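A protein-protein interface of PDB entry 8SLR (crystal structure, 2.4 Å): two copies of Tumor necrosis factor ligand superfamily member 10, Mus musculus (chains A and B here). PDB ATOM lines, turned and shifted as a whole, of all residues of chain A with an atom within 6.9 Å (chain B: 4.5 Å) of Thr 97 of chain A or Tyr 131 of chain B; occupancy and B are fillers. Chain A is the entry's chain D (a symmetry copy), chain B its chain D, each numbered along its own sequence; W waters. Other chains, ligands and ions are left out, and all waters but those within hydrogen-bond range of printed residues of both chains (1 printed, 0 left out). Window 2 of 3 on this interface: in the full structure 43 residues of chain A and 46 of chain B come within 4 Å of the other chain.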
ATOM      1  N   LEU A  25      -0.045  21.242 -21.048  1.00  0.00           N
ATOM      2  CA  LEU A  25       1.298  21.441 -21.590  1.00  0.00           C
ATOM      3  C   LEU A  25       2.299  20.477 -20.961  1.00  0.00           C
ATOM      4  O   LEU A  25       2.899  19.648 -21.657  1.00  0.00           O
ATOM      5  CB  LEU A  25       1.742  22.895 -21.386  1.00  0.00           C
ATOM      6  CG  LEU A  25       1.649  23.768 -22.640  1.00  0.00           C
ATOM      7  CD1 LEU A  25       1.711  25.244 -22.282  1.00  0.00           C
ATOM      8  CD2 LEU A  25       2.763  23.413 -23.609  1.00  0.00           C
ATOM      9  N   ILE A  26       2.521  20.599 -19.654  1.00  0.00           N
ATOM     10  CA  ILE A  26       3.276  19.614 -18.882  1.00  0.00           C
ATOM     11  C   ILE A  26       2.249  18.866 -18.037  1.00  0.00           C
ATOM     12  O   ILE A  26       1.935  19.323 -16.928  1.00  0.00           O
ATOM     13  CB  ILE A  26       4.357  20.264 -18.001  1.00  0.00           C
ATOM     14  CG1 ILE A  26       5.379  21.022 -18.841  1.00  0.00           C
ATOM     15  CG2 ILE A  26       5.107  19.200 -17.206  1.00  0.00           C
ATOM     16  CD1 ILE A  26       6.106  22.084 -18.058  1.00  0.00           C
ATOM     17  N   GLU A  82      23.034  21.416 -31.151  1.00  0.00           N
ATOM     18  CA  GLU A  82      22.160  20.950 -32.231  1.00  0.00           C
ATOM     19  C   GLU A  82      22.889  21.022 -33.568  1.00  0.00           C
ATOM     20  O   GLU A  82      23.734  20.175 -33.865  1.00  0.00           O
ATOM     21  CB  GLU A  82      20.868  21.773 -32.272  1.00  0.00           C
ATOM     22  CG  GLU A  82      19.914  21.449 -31.118  1.00  0.00           C
ATOM     23  CD  GLU A  82      18.863  22.525 -30.865  1.00  0.00           C
ATOM     24  OE1 GLU A  82      19.095  23.702 -31.211  1.00  0.00           O
ATOM     25  OE2 GLU A  82      17.798  22.192 -30.304  1.00  0.00           O
ATOM     26  N   ARG A  96      10.305  23.010 -33.233  1.00  0.00           N
ATOM     27  CA  ARG A  96      10.684  22.100 -32.157  1.00  0.00           C
ATOM     28  C   ARG A  96      11.254  22.879 -30.974  1.00  0.00           C
ATOM     29  O   ARG A  96      12.075  23.786 -31.141  1.00  0.00           O
ATOM     30  CB  ARG A  96      11.701  21.070 -32.653  1.00  0.00           C
ATOM     31  N   THR A  97      10.794  22.525 -29.777  1.00  0.00           N
ATOM     32  CA  THR A  97      11.348  23.031 -28.534  1.00  0.00           C
ATOM     33  C   THR A  97      11.521  21.859 -27.583  1.00  0.00           C
ATOM     34  O   THR A  97      10.824  20.845 -27.676  1.00  0.00           O
ATOM     35  CB  THR A  97      10.458  24.103 -27.870  1.00  0.00           C
ATOM     36  OG1 THR A  97      11.235  24.865 -26.936  1.00  0.00           O
ATOM     37  CG2 THR A  97       9.288  23.469 -27.108  1.00  0.00           C
ATOM     38  N   LYS A  98      12.439  22.031 -26.648  1.00  0.00           N
ATOM     39  CA  LYS A  98      12.666  21.071 -25.581  1.00  0.00           C
ATOM     40  C   LYS A  98      12.000  21.601 -24.316  1.00  0.00           C
ATOM     41  O   LYS A  98      12.173  22.770 -23.963  1.00  0.00           O
ATOM     42  CB  LYS A  98      14.166  20.858 -25.375  1.00  0.00           C
ATOM     43  CG  LYS A  98      14.856  20.195 -26.575  1.00  0.00           C
ATOM     44  CD  LYS A  98      16.342  20.554 -26.678  1.00  0.00           C
ATOM     45  CE  LYS A  98      16.963  20.070 -27.998  1.00  0.00           C
ATOM     46  NZ  LYS A  98      16.696  18.629 -28.288  1.00  0.00           N
ATOM     47  N   GLN A  99      11.206  20.757 -23.664  1.00  0.00           N
ATOM     48  CA  GLN A  99      10.653  21.070 -22.353  1.00  0.00           C
ATOM     49  C   GLN A  99      11.664  20.625 -21.303  1.00  0.00           C
ATOM     50  O   GLN A  99      11.916  19.426 -21.141  1.00  0.00           O
ATOM     51  CB  GLN A  99       9.304  20.388 -22.153  1.00  0.00           C
ATOM     52  CG  GLN A  99       8.279  20.733 -23.229  1.00  0.00           C
ATOM     53  CD  GLN A  99       6.878  20.266 -22.882  1.00  0.00           C
ATOM     54  OE1 GLN A  99       6.678  19.504 -21.933  1.00  0.00           O
ATOM     55  NE2 GLN A  99       5.895  20.730 -23.647  1.00  0.00           N
ATOM     56  N   ARG A 121      11.365  25.292 -18.117  1.00  0.00           N
ATOM     57  CA  ARG A 121      11.774  26.181 -19.195  1.00  0.00           C
ATOM     58  C   ARG A 121      11.505  25.491 -20.526  1.00  0.00           C
ATOM     59  O   ARG A 121      11.471  24.260 -20.611  1.00  0.00           O
ATOM     60  CB  ARG A 121      13.266  26.550 -19.145  1.00  0.00           C
ATOM     61  CG  ARG A 121      13.826  26.948 -17.796  1.00  0.00           C
ATOM     62  CD  ARG A 121      13.495  28.373 -17.395  1.00  0.00           C
ATOM     63  NE  ARG A 121      14.270  28.743 -16.213  1.00  0.00           N
ATOM     64  CZ  ARG A 121      14.050  28.293 -14.982  1.00  0.00           C
ATOM     65  NH1 ARG A 121      13.038  27.482 -14.703  1.00  0.00           N
ATOM     66  NH2 ARG A 121      14.875  28.658 -14.003  1.00  0.00           N
ATOM     67  N   ASN A 122      11.335  26.298 -21.570  1.00  0.00           N
ATOM     68  CA  ASN A 122      11.331  25.817 -22.946  1.00  0.00           C
ATOM     69  C   ASN A 122      12.558  26.395 -23.638  1.00  0.00           C
ATOM     70  O   ASN A 122      12.934  27.544 -23.393  1.00  0.00           O
ATOM     71  CB  ASN A 122      10.064  26.215 -23.708  1.00  0.00           C
ATOM     72  CG  ASN A 122      10.054  27.669 -24.095  1.00  0.00           C
ATOM     73  OD1 ASN A 122      10.511  28.058 -25.167  1.00  0.00           O
ATOM     74  ND2 ASN A 122       9.539  28.485 -23.213  1.00  0.00           N
ATOM     75  N   SER A 123      13.205  25.590 -24.469  1.00  0.00           N
ATOM     76  CA  SER A 123      14.342  26.107 -25.206  1.00  0.00           C
ATOM     77  C   SER A 123      13.875  27.087 -26.274  1.00  0.00           C
ATOM     78  O   SER A 123      12.698  27.132 -26.645  1.00  0.00           O
ATOM     79  CB  SER A 123      15.136  24.974 -25.847  1.00  0.00           C
ATOM     80  OG  SER A 123      14.292  24.142 -26.617  1.00  0.00           O
ATOM     81  N   CYS A 124      14.824  27.883 -26.762  1.00  0.00           N
ATOM     82  CA  CYS A 124      14.534  28.869 -27.791  1.00  0.00           C
ATOM     83  C   CYS A 124      13.945  28.192 -29.021  1.00  0.00           C
ATOM     84  O   CYS A 124      14.415  27.138 -29.454  1.00  0.00           O
ATOM     85  CB  CYS A 124      15.813  29.619 -28.151  1.00  0.00           C
ATOM     86  SG  CYS A 124      15.597  30.897 -29.394  1.00  0.00           S
ATOM     87  N   TRP A 125      12.886  28.797 -29.564  1.00  0.00           N
ATOM     88  CA  TRP A 125      12.179  28.252 -30.716  1.00  0.00           C
ATOM     89  C   TRP A 125      12.831  28.584 -32.050  1.00  0.00           C
ATOM     90  O   TRP A 125      12.409  28.034 -33.073  1.00  0.00           O
ATOM     91  CB  TRP A 125      10.754  28.791 -30.767  1.00  0.00           C
ATOM     92  CG  TRP A 125       9.856  28.350 -29.670  1.00  0.00           C
ATOM     93  CD1 TRP A 125       9.694  28.941 -28.454  1.00  0.00           C
ATOM     94  CD2 TRP A 125       8.943  27.248 -29.708  1.00  0.00           C
ATOM     95  NE1 TRP A 125       8.745  28.268 -27.725  1.00  0.00           N
ATOM     96  CE2 TRP A 125       8.272  27.222 -28.472  1.00  0.00           C
ATOM     97  CE3 TRP A 125       8.633  26.277 -30.666  1.00  0.00           C
ATOM     98  CZ2 TRP A 125       7.307  26.267 -28.168  1.00  0.00           C
ATOM     99  CZ3 TRP A 125       7.682  25.324 -30.360  1.00  0.00           C
ATOM    100  CH2 TRP A 125       7.032  25.324 -29.121  1.00  0.00           C
ATOM    101  N   ASN A 156      14.334  15.157 -20.199  1.00  0.00           N
ATOM    102  CA  ASN A 156      15.499  15.254 -21.087  1.00  0.00           C
ATOM    103  C   ASN A 156      16.817  15.030 -20.338  1.00  0.00           C
ATOM    104  O   ASN A 156      17.746  15.836 -20.431  1.00  0.00           O
ATOM    105  CB  ASN A 156      15.516  16.613 -21.806  1.00  0.00           C
ATOM    106  CG  ASN A 156      14.494  16.700 -22.931  1.00  0.00           C
ATOM    107  OD1 ASN A 156      14.631  16.029 -23.953  1.00  0.00           O
ATOM    108  ND2 ASN A 156      13.482  17.545 -22.760  1.00  0.00           N
ATOM    109  N   PHE B  80       1.983  29.870 -21.002  1.00  0.00           N
ATOM    110  CA  PHE B  80       1.034  30.437 -21.947  1.00  0.00           C
ATOM    111  C   PHE B  80       1.120  29.717 -23.282  1.00  0.00           C
ATOM    112  O   PHE B  80       2.152  29.143 -23.636  1.00  0.00           O
ATOM    113  CB  PHE B  80       1.267  31.942 -22.117  1.00  0.00           C
ATOM    114  CG  PHE B  80       2.660  32.313 -22.539  1.00  0.00           C
ATOM    115  CD1 PHE B  80       3.007  32.369 -23.878  1.00  0.00           C
ATOM    116  CD2 PHE B  80       3.612  32.650 -21.591  1.00  0.00           C
ATOM    117  CE1 PHE B  80       4.281  32.731 -24.261  1.00  0.00           C
ATOM    118  CE2 PHE B  80       4.888  33.011 -21.970  1.00  0.00           C
ATOM    119  CZ  PHE B  80       5.220  33.059 -23.308  1.00  0.00           C
ATOM    120  N   GLN B  81       0.004  29.738 -24.003  1.00  0.00           N
ATOM    121  CA  GLN B  81      -0.111  29.190 -25.345  1.00  0.00           C
ATOM    122  C   GLN B  81      -0.480  30.323 -26.291  1.00  0.00           C
ATOM    123  O   GLN B  81      -1.266  31.206 -25.932  1.00  0.00           O
ATOM    124  CB  GLN B  81      -1.171  28.082 -25.387  1.00  0.00           C
ATOM    125  CG  GLN B  81      -1.184  27.247 -26.665  1.00  0.00           C
ATOM    126  CD  GLN B  81      -0.295  26.019 -26.585  1.00  0.00           C
ATOM    127  OE1 GLN B  81      -0.226  25.348 -25.552  1.00  0.00           O
ATOM    128  NE2 GLN B  81       0.390  25.712 -27.685  1.00  0.00           N
ATOM    129  N   ALA B 129       7.219  30.721 -31.986  1.00  0.00           N
ATOM    130  CA  ALA B 129       6.961  30.376 -30.588  1.00  0.00           C
ATOM    131  C   ALA B 129       5.500  29.981 -30.406  1.00  0.00           C
ATOM    132  O   ALA B 129       4.603  30.825 -30.488  1.00  0.00           O
ATOM    133  CB  ALA B 129       7.330  31.544 -29.677  1.00  0.00           C
ATOM    134  N   GLU B 130       5.263  28.696 -30.140  1.00  0.00           N
ATOM    135  CA  GLU B 130       3.906  28.205 -29.923  1.00  0.00           C
ATOM    136  C   GLU B 130       3.464  28.379 -28.476  1.00  0.00           C
ATOM    137  O   GLU B 130       2.285  28.644 -28.215  1.00  0.00           O
ATOM    138  CB  GLU B 130       3.808  26.728 -30.307  1.00  0.00           C
ATOM    139  CG  GLU B 130       4.153  26.418 -31.753  1.00  0.00           C
ATOM    140  CD  GLU B 130       4.036  24.937 -32.069  1.00  0.00           C
ATOM    141  OE1 GLU B 130       3.546  24.174 -31.203  1.00  0.00           O
ATOM    142  OE2 GLU B 130       4.445  24.534 -33.179  1.00  0.00           O
ATOM    143  N   TYR B 131       4.381  28.210 -27.524  1.00  0.00           N
ATOM    144  CA  TYR B 131       4.042  28.332 -26.116  1.00  0.00           C
ATOM    145  C   TYR B 131       5.273  28.748 -25.326  1.00  0.00           C
ATOM    146  O   TYR B 131       6.393  28.790 -25.847  1.00  0.00           O
ATOM    147  CB  TYR B 131       3.459  27.026 -25.569  1.00  0.00           C
ATOM    148  CG  TYR B 131       4.374  25.822 -25.629  1.00  0.00           C
ATOM    149  CD1 TYR B 131       5.300  25.574 -24.623  1.00  0.00           C
ATOM    150  CD2 TYR B 131       4.280  24.909 -26.667  1.00  0.00           C
ATOM    151  CE1 TYR B 131       6.122  24.464 -24.666  1.00  0.00           C
ATOM    152  CE2 TYR B 131       5.098  23.796 -26.716  1.00  0.00           C
ATOM    153  CZ  TYR B 131       6.014  23.578 -25.712  1.00  0.00           C
ATOM    154  OH  TYR B 131       6.836  22.475 -25.747  1.00  0.00           O
ATOM    155  N   GLY B 132       5.043  29.047 -24.054  1.00  0.00           N
ATOM    156  CA  GLY B 132       6.103  29.489 -23.170  1.00  0.00           C
ATOM    157  C   GLY B 132       5.969  28.876 -21.794  1.00  0.00           C
ATOM    158  O   GLY B 132       4.870  28.658 -21.286  1.00  0.00           O
ATOM    159  N   LEU B 133       7.124  28.637 -21.183  1.00  0.00           N
ATOM    160  CA  LEU B 133       7.263  28.031 -19.864  1.00  0.00           C
ATOM    161  C   LEU B 133       8.393  28.797 -19.198  1.00  0.00           C
ATOM    162  O   LEU B 133       9.543  28.675 -19.626  1.00  0.00           O
ATOM    163  CB  LEU B 133       7.603  26.546 -19.947  1.00  0.00           C
ATOM    164  CG  LEU B 133       6.679  25.651 -20.767  1.00  0.00           C
ATOM    165  CD1 LEU B 133       7.330  24.296 -20.914  1.00  0.00           C
ATOM    166  CD2 LEU B 133       5.331  25.518 -20.113  1.00  0.00           C
HETATM  167  O   HOH W   1      12.194  29.383 -20.783  1.00  0.00           O
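The side-chain hydroxyl of Tyr 131 of chain B is in hydrogen-bond range of the side-chain amide nitrogen of Gln 99 of chain A, 2.9 Å away.
The backbone carbonyl oxygen (O) of Tyr 131 of chain B is in hydrogen-bond range of the indole nitrogen (NE1) of Trp 125 of chain A (3.1 Å).
The backbone NH (N) of Leu 133 of chain B lies close to the side-chain amide nitrogen (ND2) of Asn 122 of chain A.
The side-chain amide nitrogen (ND2) of Asn 156 of chain A lies within hydrogen-bond range of the backbone carbonyl oxygen (O) of Gln 99 of chain A (2.9 Å).
O of Phe 80 of chain B is in hydrogen-bond range of N of Gly 132 of chain B, 2.9 Å away.
The indole nitrogen (NE1) of Trp 125 of chain A lies within hydrogen-bond range of the side-chain amide oxygen (OD1) of Asn 122 of chain A (3.1 Å).
OG1 of Thr 97 of chain A is in hydrogen-bond range of O of Ser 123 of chain A.
Leu 25 of chain A touches Gln 81 of chain B.
CD1 of Tyr 131 of chain B touches CD2 of Leu 25 of chain A, 3.5 Å away.
Leu 133 of chain B touches Ile 26 of chain A.
Thr 97 of chain A touches Tyr 131 of chain B.
Leu 133 of chain B touches Arg 121 of chain A (O to CA, 3.4 Å).
ND2 of Asn 122 of chain A touches CA of Gly 132 of chain B (3.6 Å).
CG of Trp 125 of chain A touches CA of Ala 129 of chain B (3.7 Å).
Glu 130 of chain B touches Trp 125 of chain A.
Of chain B, only Tyr 131 (3.0 Å) comes within 4 Å of Thr 97 of chain A.
Tyr 131 of chain B touches four residues of chain A.
Of the printed residues of chain B, Gln 99 of chain A touches Tyr 131.
Of the printed residues of chain A, Ala 129 of chain B touches Trp 125 (3.7 Å).
Printed residues of chain A within 4 Å of Gln 81 of chain B: Leu 25 (3.8 Å).
Of the printed residues of chain A, Leu 133 of chain B touches Ile 26, Arg 121 and Asn 122.
Of the printed residues of chain B, Ile 26 of chain A touches Leu 133 (3.8 Å).
Arg 96 of chain A touches none of the printed residues of chain B.
The nearest printed residue of chain B that does not touch Thr 97 of chain A is Leu 133 of chain B (6.5 Å).
Printed residues of chain B that touch a printed residue of chain A: Gln 81, Ala 129, Glu 130, Tyr 131, Gly 132 and Leu 133.
Hydrophobic or aromatic side chains of chain B that line the printed part of chain A: Ala 129, Tyr 131 and Leu 133.
Along chain A the printed residues that touch a printed residue of chain B span positions 25 to 125.
No position is printed for both chains.
Water W1 bridges O of Leu 133 of chain B (3.0 Å) and O of Asn 122 of chain A (3.3 Å).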
